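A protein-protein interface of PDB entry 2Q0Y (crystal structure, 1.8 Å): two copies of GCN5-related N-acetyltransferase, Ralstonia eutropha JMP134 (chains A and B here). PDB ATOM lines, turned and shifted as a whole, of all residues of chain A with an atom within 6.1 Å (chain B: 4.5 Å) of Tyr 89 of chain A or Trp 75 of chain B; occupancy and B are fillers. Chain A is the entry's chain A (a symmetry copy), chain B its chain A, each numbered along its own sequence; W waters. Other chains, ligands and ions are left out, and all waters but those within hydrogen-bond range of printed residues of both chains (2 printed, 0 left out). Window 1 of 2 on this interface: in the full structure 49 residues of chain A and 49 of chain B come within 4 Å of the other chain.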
ATOM      1  N   ARG A  19      10.500  18.146   7.768  1.00  0.00           N
ATOM      2  CA  ARG A  19      11.034  18.427   6.451  1.00  0.00           C
ATOM      3  C   ARG A  19      12.540  18.653   6.511  1.00  0.00           C
ATOM      4  O   ARG A  19      13.281  18.075   5.724  1.00  0.00           O
ATOM      5  CB  ARG A  19      10.332  19.635   5.837  1.00  0.00           C
ATOM      6  CG  ARG A  19      10.729  19.941   4.396  1.00  0.00           C
ATOM      7  CD  ARG A  19       9.785  20.927   3.768  1.00  0.00           C
ATOM      8  NE  ARG A  19      10.046  21.180   2.350  1.00  0.00           N
ATOM      9  CZ  ARG A  19       9.649  20.403   1.345  1.00  0.00           C
ATOM     10  NH1 ARG A  19       9.025  19.255   1.574  1.00  0.00           N
ATOM     11  NH2 ARG A  19       9.927  20.741   0.106  1.00  0.00           N
ATOM     12  N   TRP A  43       4.749  29.164   3.211  1.00  0.00           N
ATOM     13  CA  TRP A  43       3.980  28.387   2.245  1.00  0.00           C
ATOM     14  C   TRP A  43       3.005  27.463   2.983  1.00  0.00           C
ATOM     15  O   TRP A  43       1.859  27.311   2.565  1.00  0.00           O
ATOM     16  CB  TRP A  43       4.924  27.562   1.365  1.00  0.00           C
ATOM     17  CG  TRP A  43       4.259  26.609   0.403  1.00  0.00           C
ATOM     18  CD1 TRP A  43       3.871  26.872  -0.883  1.00  0.00           C
ATOM     19  CD2 TRP A  43       3.930  25.235   0.647  1.00  0.00           C
ATOM     20  NE1 TRP A  43       3.317  25.754  -1.447  1.00  0.00           N
ATOM     21  CE2 TRP A  43       3.324  24.738  -0.530  1.00  0.00           C
ATOM     22  CE3 TRP A  43       4.067  24.389   1.745  1.00  0.00           C
ATOM     23  CZ2 TRP A  43       2.875  23.446  -0.634  1.00  0.00           C
ATOM     24  CZ3 TRP A  43       3.603  23.104   1.652  1.00  0.00           C
ATOM     25  CH2 TRP A  43       3.011  22.639   0.475  1.00  0.00           C
ATOM     26  N   GLY A  69       2.967  13.913   5.179  1.00  0.00           N
ATOM     27  CA  GLY A  69       2.157  14.940   4.531  1.00  0.00           C
ATOM     28  C   GLY A  69       1.535  14.406   3.256  1.00  0.00           C
ATOM     29  O   GLY A  69       2.126  13.554   2.581  1.00  0.00           O
ATOM     30  N   LEU A  70       0.366  14.932   2.901  1.00  0.00           N
ATOM     31  CA  LEU A  70      -0.289  14.575   1.653  1.00  0.00           C
ATOM     32  C   LEU A  70      -1.050  15.753   1.058  1.00  0.00           C
ATOM     33  O   LEU A  70      -1.583  16.596   1.768  1.00  0.00           O
ATOM     34  CB  LEU A  70      -1.209  13.357   1.831  1.00  0.00           C
ATOM     35  CG  LEU A  70      -2.475  13.427   2.666  1.00  0.00           C
ATOM     36  CD1 LEU A  70      -3.728  13.844   1.847  1.00  0.00           C
ATOM     37  CD2 LEU A  70      -2.727  12.049   3.332  1.00  0.00           C
ATOM     38  N   MET A  71      -1.050  15.788  -0.265  1.00  0.00           N
ATOM     39  CA  MET A  71      -1.731  16.800  -1.041  1.00  0.00           C
ATOM     40  C   MET A  71      -2.388  16.121  -2.220  1.00  0.00           C
ATOM     41  O   MET A  71      -2.014  15.016  -2.598  1.00  0.00           O
ATOM     42  CB  MET A  71      -0.728  17.832  -1.545  1.00  0.00           C
ATOM     43  CG  MET A  71       0.122  18.457  -0.452  1.00  0.00           C
ATOM     44  SD  MET A  71       1.469  19.597  -1.236  1.00  0.00           S
ATOM     45  CE  MET A  71       0.347  20.885  -1.570  1.00  0.00           C
ATOM     46  N   VAL A  72      -3.397  16.777  -2.768  1.00  0.00           N
ATOM     47  CA  VAL A  72      -3.980  16.370  -4.042  1.00  0.00           C
ATOM     48  C   VAL A  72      -3.697  17.554  -4.952  1.00  0.00           C
ATOM     49  O   VAL A  72      -4.236  18.644  -4.749  1.00  0.00           O
ATOM     50  CB  VAL A  72      -5.475  16.078  -3.919  1.00  0.00           C
ATOM     51  CG1 VAL A  72      -6.076  15.716  -5.275  1.00  0.00           C
ATOM     52  CG2 VAL A  72      -5.703  14.952  -2.928  1.00  0.00           C
ATOM     53  N   ILE A  73      -2.803  17.361  -5.912  1.00  0.00           N
ATOM     54  CA  ILE A  73      -2.357  18.453  -6.759  1.00  0.00           C
ATOM     55  C   ILE A  73      -3.064  18.442  -8.097  1.00  0.00           C
ATOM     56  O   ILE A  73      -3.419  17.380  -8.619  1.00  0.00           O
ATOM     57  CB  ILE A  73      -0.842  18.449  -6.933  1.00  0.00           C
ATOM     58  CG1 ILE A  73      -0.359  17.203  -7.654  1.00  0.00           C
ATOM     59  CG2 ILE A  73      -0.174  18.518  -5.544  1.00  0.00           C
ATOM     60  CD1 ILE A  73       1.142  17.205  -7.935  1.00  0.00           C
ATOM     61  N   TRP A  75      -3.342  18.423 -11.975  1.00  0.00           N
ATOM     62  CA  TRP A  75      -2.528  17.785 -12.979  1.00  0.00           C
ATOM     63  C   TRP A  75      -3.357  17.533 -14.239  1.00  0.00           C
ATOM     64  O   TRP A  75      -4.526  17.204 -14.134  1.00  0.00           O
ATOM     65  CB  TRP A  75      -1.959  16.464 -12.459  1.00  0.00           C
ATOM     66  CG  TRP A  75      -0.724  16.099 -13.147  1.00  0.00           C
ATOM     67  CD1 TRP A  75      -0.588  15.287 -14.226  1.00  0.00           C
ATOM     68  CD2 TRP A  75       0.580  16.602 -12.853  1.00  0.00           C
ATOM     69  NE1 TRP A  75       0.732  15.240 -14.622  1.00  0.00           N
ATOM     70  CE2 TRP A  75       1.468  16.041 -13.794  1.00  0.00           C
ATOM     71  CE3 TRP A  75       1.080  17.476 -11.886  1.00  0.00           C
ATOM     72  CZ2 TRP A  75       2.833  16.319 -13.791  1.00  0.00           C
ATOM     73  CZ3 TRP A  75       2.439  17.767 -11.895  1.00  0.00           C
ATOM     74  CH2 TRP A  75       3.295  17.176 -12.823  1.00  0.00           C
ATOM     75  N   ARG A  87      -3.573  14.429  -9.141  1.00  0.00           N
ATOM     76  CA  ARG A  87      -2.895  13.267  -8.608  1.00  0.00           C
ATOM     77  C   ARG A  87      -2.549  13.485  -7.132  1.00  0.00           C
ATOM     78  O   ARG A  87      -2.470  14.623  -6.658  1.00  0.00           O
ATOM     79  CB  ARG A  87      -1.684  12.861  -9.468  1.00  0.00           C
ATOM     80  CG  ARG A  87      -0.739  13.927  -9.806  1.00  0.00           C
ATOM     81  CD  ARG A  87       0.489  13.371 -10.576  1.00  0.00           C
ATOM     82  NE  ARG A  87       0.200  12.850 -11.915  1.00  0.00           N
ATOM     83  CZ  ARG A  87       1.132  12.438 -12.777  1.00  0.00           C
ATOM     84  NH1 ARG A  87       2.421  12.518 -12.468  1.00  0.00           N
ATOM     85  NH2 ARG A  87       0.799  11.963 -13.965  1.00  0.00           N
ATOM     86  N   GLY A  88      -2.417  12.386  -6.406  1.00  0.00           N
ATOM     87  CA  GLY A  88      -1.992  12.431  -5.018  1.00  0.00           C
ATOM     88  C   GLY A  88      -0.504  12.694  -4.936  1.00  0.00           C
ATOM     89  O   GLY A  88       0.263  12.304  -5.826  1.00  0.00           O
ATOM     90  N   TYR A  89      -0.091  13.376  -3.871  1.00  0.00           N
ATOM     91  CA  TYR A  89       1.317  13.653  -3.626  1.00  0.00           C
ATOM     92  C   TYR A  89       1.618  13.424  -2.141  1.00  0.00           C
ATOM     93  O   TYR A  89       0.914  13.946  -1.277  1.00  0.00           O
ATOM     94  CB  TYR A  89       1.702  15.084  -4.058  1.00  0.00           C
ATOM     95  CG  TYR A  89       3.191  15.319  -3.919  1.00  0.00           C
ATOM     96  CD1 TYR A  89       4.095  14.514  -4.614  1.00  0.00           C
ATOM     97  CD2 TYR A  89       3.703  16.318  -3.107  1.00  0.00           C
ATOM     98  CE1 TYR A  89       5.452  14.675  -4.487  1.00  0.00           C
ATOM     99  CE2 TYR A  89       5.087  16.488  -2.977  1.00  0.00           C
ATOM    100  CZ  TYR A  89       5.956  15.655  -3.665  1.00  0.00           C
ATOM    101  OH  TYR A  89       7.356  15.784  -3.576  1.00  0.00           O
ATOM    102  N   ILE A  90       2.633  12.622  -1.870  1.00  0.00           N
ATOM    103  CA  ILE A  90       3.081  12.332  -0.514  1.00  0.00           C
ATOM    104  C   ILE A  90       4.423  13.013  -0.306  1.00  0.00           C
ATOM    105  O   ILE A  90       5.297  12.960  -1.169  1.00  0.00           O
ATOM    106  CB  ILE A  90       3.192  10.800  -0.265  1.00  0.00           C
ATOM    107  CG1 ILE A  90       1.813  10.156  -0.425  1.00  0.00           C
ATOM    108  CG2 ILE A  90       3.798  10.504   1.116  1.00  0.00           C
ATOM    109  CD1 ILE A  90       1.798   8.667  -0.296  1.00  0.00           C
ATOM    110  N   LEU A  91       4.575  13.657   0.844  1.00  0.00           N
ATOM    111  CA  LEU A  91       5.799  14.365   1.174  1.00  0.00           C
ATOM    112  C   LEU A  91       6.036  14.428   2.680  1.00  0.00           C
ATOM    113  O   LEU A  91       5.123  14.186   3.488  1.00  0.00           O
ATOM    114  CB  LEU A  91       5.808  15.786   0.581  1.00  0.00           C
ATOM    115  CG  LEU A  91       4.869  16.839   1.160  1.00  0.00           C
ATOM    116  CD1 LEU A  91       5.259  18.239   0.708  1.00  0.00           C
ATOM    117  CD2 LEU A  91       3.399  16.561   0.848  1.00  0.00           C
ATOM    118  N   PHE A 116      -6.022   8.705   0.194  1.00  0.00           N
ATOM    119  CA  PHE A 116      -6.196   8.906  -1.248  1.00  0.00           C
ATOM    120  C   PHE A 116      -7.323   8.018  -1.800  1.00  0.00           C
ATOM    121  O   PHE A 116      -8.126   8.462  -2.618  1.00  0.00           O
ATOM    122  CB  PHE A 116      -4.900   8.612  -2.023  1.00  0.00           C
ATOM    123  CG  PHE A 116      -3.815   9.642  -1.850  1.00  0.00           C
ATOM    124  CD1 PHE A 116      -4.101  11.000  -1.713  1.00  0.00           C
ATOM    125  CD2 PHE A 116      -2.495   9.244  -1.855  1.00  0.00           C
ATOM    126  CE1 PHE A 116      -3.092  11.925  -1.558  1.00  0.00           C
ATOM    127  CE2 PHE A 116      -1.471  10.182  -1.691  1.00  0.00           C
ATOM    128  CZ  PHE A 116      -1.781  11.519  -1.548  1.00  0.00           C
ATOM    129  N   PHE A 123      -4.243   7.988  -8.830  1.00  0.00           N
ATOM    130  CA  PHE A 123      -2.790   7.845  -9.014  1.00  0.00           C
ATOM    131  C   PHE A 123      -2.079   8.795  -8.072  1.00  0.00           C
ATOM    132  O   PHE A 123      -2.549   9.915  -7.859  1.00  0.00           O
ATOM    133  CB  PHE A 123      -2.474   8.185 -10.476  1.00  0.00           C
ATOM    134  CG  PHE A 123      -1.062   7.906 -10.912  1.00  0.00           C
ATOM    135  CD1 PHE A 123      -0.616   6.607 -11.098  1.00  0.00           C
ATOM    136  CD2 PHE A 123      -0.198   8.955 -11.194  1.00  0.00           C
ATOM    137  CE1 PHE A 123       0.678   6.368 -11.545  1.00  0.00           C
ATOM    138  CE2 PHE A 123       1.093   8.701 -11.654  1.00  0.00           C
ATOM    139  CZ  PHE A 123       1.510   7.411 -11.821  1.00  0.00           C
ATOM    140  N   ALA A 124      -0.947   8.358  -7.529  1.00  0.00           N
ATOM    141  CA  ALA A 124      -0.161   9.187  -6.622  1.00  0.00           C
ATOM    142  C   ALA A 124       1.323   9.089  -6.924  1.00  0.00           C
ATOM    143  O   ALA A 124       1.799   8.088  -7.513  1.00  0.00           O
ATOM    144  CB  ALA A 124      -0.423   8.763  -5.190  1.00  0.00           C
ATOM    145  N   VAL A 125       2.047  10.123  -6.505  1.00  0.00           N
ATOM    146  CA  VAL A 125       3.494  10.196  -6.680  1.00  0.00           C
ATOM    147  C   VAL A 125       4.141  10.693  -5.394  1.00  0.00           C
ATOM    148  O   VAL A 125       3.472  11.223  -4.513  1.00  0.00           O
ATOM    149  CB  VAL A 125       3.915  11.106  -7.868  1.00  0.00           C
ATOM    150  CG1 VAL A 125       3.398  10.556  -9.210  1.00  0.00           C
ATOM    151  CG2 VAL A 125       3.445  12.521  -7.664  1.00  0.00           C
ATOM    152  N   LEU A 126       5.445  10.461  -5.283  1.00  0.00           N
ATOM    153  CA  LEU A 126       6.257  10.940  -4.162  1.00  0.00           C
ATOM    154  C   LEU A 126       7.673  11.102  -4.683  1.00  0.00           C
ATOM    155  O   LEU A 126       7.997  10.555  -5.733  1.00  0.00           O
ATOM    156  CB  LEU A 126       6.205   9.948  -2.979  1.00  0.00           C
ATOM    157  CG  LEU A 126       6.670   8.496  -3.147  1.00  0.00           C
ATOM    158  CD1 LEU A 126       8.196   8.333  -3.142  1.00  0.00           C
ATOM    159  CD2 LEU A 126       6.054   7.635  -2.053  1.00  0.00           C
ATOM    160  N   HIS A 127       8.511  11.854  -3.975  1.00  0.00           N
ATOM    161  CA  HIS A 127       9.936  11.905  -4.290  1.00  0.00           C
ATOM    162  C   HIS A 127      10.690  11.246  -3.158  1.00  0.00           C
ATOM    163  O   HIS A 127      10.633  11.704  -2.008  1.00  0.00           O
ATOM    164  CB  HIS A 127      10.390  13.336  -4.508  1.00  0.00           C
ATOM    165  CG  HIS A 127       9.826  13.953  -5.746  1.00  0.00           C
ATOM    166  ND1 HIS A 127       8.694  14.733  -5.734  1.00  0.00           N
ATOM    167  CD2 HIS A 127      10.239  13.909  -7.033  1.00  0.00           C
ATOM    168  CE1 HIS A 127       8.433  15.148  -6.961  1.00  0.00           C
ATOM    169  NE2 HIS A 127       9.348  14.649  -7.771  1.00  0.00           N
ATOM    170  N   ILE B  73       4.271  25.469 -12.113  1.00  0.00           N
ATOM    171  CA  ILE B  73       3.352  24.869 -11.161  1.00  0.00           C
ATOM    172  C   ILE B  73       3.684  25.270  -9.740  1.00  0.00           C
ATOM    173  O   ILE B  73       4.851  25.486  -9.398  1.00  0.00           O
ATOM    174  CB  ILE B  73       3.297  23.352 -11.310  1.00  0.00           C
ATOM    175  CG1 ILE B  73       4.632  22.704 -10.991  1.00  0.00           C
ATOM    176  CG2 ILE B  73       2.900  23.001 -12.759  1.00  0.00           C
ATOM    177  CD1 ILE B  73       4.595  21.178 -11.033  1.00  0.00           C
ATOM    178  N   GLU B  74       2.648  25.371  -8.913  1.00  0.00           N
ATOM    179  CA  GLU B  74       2.840  25.618  -7.491  1.00  0.00           C
ATOM    180  C   GLU B  74       3.558  24.428  -6.862  1.00  0.00           C
ATOM    181  O   GLU B  74       3.260  23.290  -7.180  1.00  0.00           O
ATOM    182  CB  GLU B  74       1.492  25.843  -6.808  1.00  0.00           C
ATOM    183  CG  GLU B  74       0.840  27.142  -7.192  1.00  0.00           C
ATOM    184  CD  GLU B  74      -0.380  27.464  -6.327  1.00  0.00           C
ATOM    185  OE1 GLU B  74      -0.846  26.567  -5.578  1.00  0.00           O
ATOM    186  OE2 GLU B  74      -0.859  28.624  -6.399  1.00  0.00           O
ATOM    187  N   TRP B  75       4.523  24.705  -5.987  1.00  0.00           N
ATOM    188  CA  TRP B  75       5.303  23.682  -5.335  1.00  0.00           C
ATOM    189  C   TRP B  75       5.862  24.215  -4.015  1.00  0.00           C
ATOM    190  O   TRP B  75       6.234  25.374  -3.944  1.00  0.00           O
ATOM    191  CB  TRP B  75       6.450  23.217  -6.234  1.00  0.00           C
ATOM    192  CG  TRP B  75       6.871  21.857  -5.911  1.00  0.00           C
ATOM    193  CD1 TRP B  75       7.878  21.478  -5.086  1.00  0.00           C
ATOM    194  CD2 TRP B  75       6.237  20.656  -6.354  1.00  0.00           C
ATOM    195  NE1 TRP B  75       7.924  20.103  -4.991  1.00  0.00           N
ATOM    196  CE2 TRP B  75       6.924  19.576  -5.761  1.00  0.00           C
ATOM    197  CE3 TRP B  75       5.153  20.391  -7.192  1.00  0.00           C
ATOM    198  CZ2 TRP B  75       6.567  18.249  -5.986  1.00  0.00           C
ATOM    199  CZ3 TRP B  75       4.785  19.067  -7.402  1.00  0.00           C
ATOM    200  CH2 TRP B  75       5.501  18.021  -6.821  1.00  0.00           C
ATOM    201  N   PRO B  76       5.935  23.372  -2.970  1.00  0.00           N
ATOM    202  CA  PRO B  76       6.584  23.874  -1.741  1.00  0.00           C
ATOM    203  C   PRO B  76       8.044  24.259  -1.953  1.00  0.00           C
ATOM    204  O   PRO B  76       8.771  23.561  -2.675  1.00  0.00           O
ATOM    205  CB  PRO B  76       6.522  22.671  -0.788  1.00  0.00           C
ATOM    206  CG  PRO B  76       6.334  21.482  -1.706  1.00  0.00           C
ATOM    207  CD  PRO B  76       5.467  21.987  -2.802  1.00  0.00           C
ATOM    208  N   PRO B  77       8.489  25.350  -1.313  1.00  0.00           N
ATOM    209  CA  PRO B  77       9.928  25.629  -1.314  1.00  0.00           C
ATOM    210  C   PRO B  77      10.700  24.366  -0.967  1.00  0.00           C
ATOM    211  O   PRO B  77      10.264  23.579  -0.113  1.00  0.00           O
ATOM    212  CB  PRO B  77      10.058  26.718  -0.250  1.00  0.00           C
ATOM    213  CG  PRO B  77       8.768  27.479  -0.425  1.00  0.00           C
ATOM    214  CD  PRO B  77       7.735  26.395  -0.606  1.00  0.00           C
ATOM    215  N   HIS B  81      15.152  24.654  -4.935  1.00  0.00           N
ATOM    216  CA  HIS B  81      14.608  25.988  -5.192  1.00  0.00           C
ATOM    217  C   HIS B  81      14.140  26.573  -3.855  1.00  0.00           C
ATOM    218  O   HIS B  81      12.942  26.764  -3.608  1.00  0.00           O
ATOM    219  CB  HIS B  81      13.512  25.983  -6.278  1.00  0.00           C
ATOM    220  CG  HIS B  81      12.412  24.987  -6.074  1.00  0.00           C
ATOM    221  ND1 HIS B  81      11.252  25.292  -5.391  1.00  0.00           N
ATOM    222  CD2 HIS B  81      12.257  23.723  -6.537  1.00  0.00           C
ATOM    223  CE1 HIS B  81      10.445  24.242  -5.421  1.00  0.00           C
ATOM    224  NE2 HIS B  81      11.033  23.279  -6.110  1.00  0.00           N
ATOM    225  N   GLN B  84      11.797  29.627  -3.763  1.00  0.00           N
ATOM    226  CA  GLN B  84      10.648  29.706  -4.672  1.00  0.00           C
ATOM    227  C   GLN B  84       9.593  28.638  -4.365  1.00  0.00           C
ATOM    228  O   GLN B  84       9.911  27.472  -4.160  1.00  0.00           O
ATOM    229  CB  GLN B  84      11.121  29.537  -6.118  1.00  0.00           C
ATOM    230  CG  GLN B  84      12.033  30.636  -6.600  1.00  0.00           C
ATOM    231  CD  GLN B  84      12.296  30.611  -8.093  1.00  0.00           C
ATOM    232  OE1 GLN B  84      11.830  29.722  -8.807  1.00  0.00           O
ATOM    233  NE2 GLN B  84      13.065  31.591  -8.571  1.00  0.00           N
ATOM    234  N   ASP B  85       8.333  29.053  -4.374  1.00  0.00           N
ATOM    235  CA  ASP B  85       7.212  28.143  -4.167  1.00  0.00           C
ATOM    236  C   ASP B  85       6.606  27.717  -5.518  1.00  0.00           C
ATOM    237  O   ASP B  85       5.376  27.675  -5.705  1.00  0.00           O
ATOM    238  CB  ASP B  85       6.149  28.785  -3.268  1.00  0.00           C
ATOM    239  CG  ASP B  85       5.577  30.071  -3.844  1.00  0.00           C
ATOM    240  OD1 ASP B  85       6.101  30.595  -4.862  1.00  0.00           O
ATOM    241  OD2 ASP B  85       4.605  30.569  -3.256  1.00  0.00           O
ATOM    242  N   LYS B  86       7.487  27.396  -6.454  1.00  0.00           N
ATOM    243  CA  LYS B  86       7.090  27.022  -7.806  1.00  0.00           C
ATOM    244  C   LYS B  86       8.211  26.218  -8.462  1.00  0.00           C
ATOM    245  O   LYS B  86       9.373  26.264  -8.021  1.00  0.00           O
ATOM    246  CB  LYS B  86       6.759  28.260  -8.641  1.00  0.00           C
ATOM    247  CG  LYS B  86       7.913  29.225  -8.816  1.00  0.00           C
ATOM    248  CD  LYS B  86       7.455  30.602  -9.321  1.00  0.00           C
ATOM    249  CE  LYS B  86       8.608  31.628  -9.321  1.00  0.00           C
ATOM    250  NZ  LYS B  86       8.176  32.965  -9.877  1.00  0.00           N
ATOM    251  N   ARG B  87       7.850  25.474  -9.504  1.00  0.00           N
ATOM    252  CA  ARG B  87       8.832  24.908 -10.404  1.00  0.00           C
ATOM    253  C   ARG B  87       8.291  24.892 -11.838  1.00  0.00           C
ATOM    254  O   ARG B  87       7.077  24.937 -12.061  1.00  0.00           O
ATOM    255  CB  ARG B  87       9.330  23.534  -9.922  1.00  0.00           C
ATOM    256  CG  ARG B  87       8.301  22.555  -9.565  1.00  0.00           C
ATOM    257  CD  ARG B  87       8.926  21.182  -9.205  1.00  0.00           C
ATOM    258  NE  ARG B  87       9.730  21.166  -7.980  1.00  0.00           N
ATOM    259  CZ  ARG B  87      10.252  20.063  -7.439  1.00  0.00           C
ATOM    260  NH1 ARG B  87      10.030  18.873  -7.984  1.00  0.00           N
ATOM    261  NH2 ARG B  87      10.983  20.124  -6.339  1.00  0.00           N
HETATM  262  O   HOH W   1       3.017  27.272  -4.222  1.00  0.00           O
HETATM  263  O   HOH W   2       2.032  24.028  -3.801  1.00  0.00           O
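NH2 of Arg 19 of chain A lies within hydrogen-bond range of O of Pro 77 of chain B (2.9 Å).
The backbone NH of Trp 75 of chain B sits at hydrogen-bond distance from the backbone carbonyl oxygen of Asp 85 of chain B (3.1 Å). O of Trp 75 of chain B lies within hydrogen-bond range of N of Lys 86 of chain B (3.5 Å). The backbone carbonyl oxygen (O) of Met 71 of chain A sits at hydrogen-bond distance from the backbone NH (N) of Tyr 89 of chain A (2.8 Å). A ring nitrogen (ND1) of His 127 of chain A is in hydrogen-bond range of the side-chain hydroxyl of Tyr 89 of chain A (2.7 Å).
O of Trp 75 of chain B touches NE1 of Trp 43 of chain A (3.9 Å). Pro 76 of chain B touches Trp 43 of chain A. Pro 77 of chain B touches Trp 43 of chain A (CD to CG, 3.6 Å). Asp 85 of chain B touches Trp 43 of chain A (CB to CD1, 3.8 Å). CZ2 of Trp 75 of chain B touches CZ of Tyr 89 of chain A, at 3.5 Å. His 127 of chain A touches Trp 75 of chain B.
Of the printed residues of chain B, Arg 19 of chain A touches Pro 77 (2.9 Å). Printed residues of chain B within 4 Å of Trp 43 of chain A: Trp 75 (3.9 Å), Pro 76 (3.6 Å), Pro 77 (3.6 Å) and Asp 85 (3.8 Å). Of chain B, only Trp 75 (3.5 Å) comes within 4 Å of Tyr 89 of chain A. Val 125 of chain A touches none of the printed residues of chain B. Of the printed residues of chain B, His 127 of chain A touches Trp 75 (3.7 Å). Trp 75 of chain B touches just these residues of chain A: Trp 43 (3.9 Å), Tyr 89 (3.5 Å) and His 127 (3.7 Å). Printed residues of chain A within 4 Å of Pro 76 of chain B: Trp 43 (3.6 Å). Of the printed residues of chain A, Pro 77 of chain B touches Arg 19 (2.9 Å) and Trp 43 (3.6 Å). The nearest printed residue of chain B that does not touch Tyr 89 of chain A is Pro 76 of chain B (5.3 Å). The nearest residue of chain A that does not touch Trp 75 of chain B is Ile 73 of chain A (4.1 Å). The nearest printed residue of chain A that does not touch Asp 85 of chain B is Arg 19 of chain A (9.0 Å).
Along chain A the printed residues that touch a printed residue of chain B span positions 19 to 127. Hydrophobic or aromatic side chains of chain B that line the printed part of chain A: Trp 75, Pro 76 and Pro 77.
3 positions are printed for both chains. Of the 7 pairs that touch across the chains among the printed residues, none has its exchanged pair printed and touching as well.
Water W1 lies within hydrogen-bond range of O of Asp 85 of chain B (2.8 Å), NE1 of Trp 43 of chain A (3.2 Å) and N of Trp 75 of chain B (3.5 Å). Water W2 bridges the indole nitrogen (NE1) of Trp 43 of chain A and the backbone NH (N) of Trp 75 of chain B.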
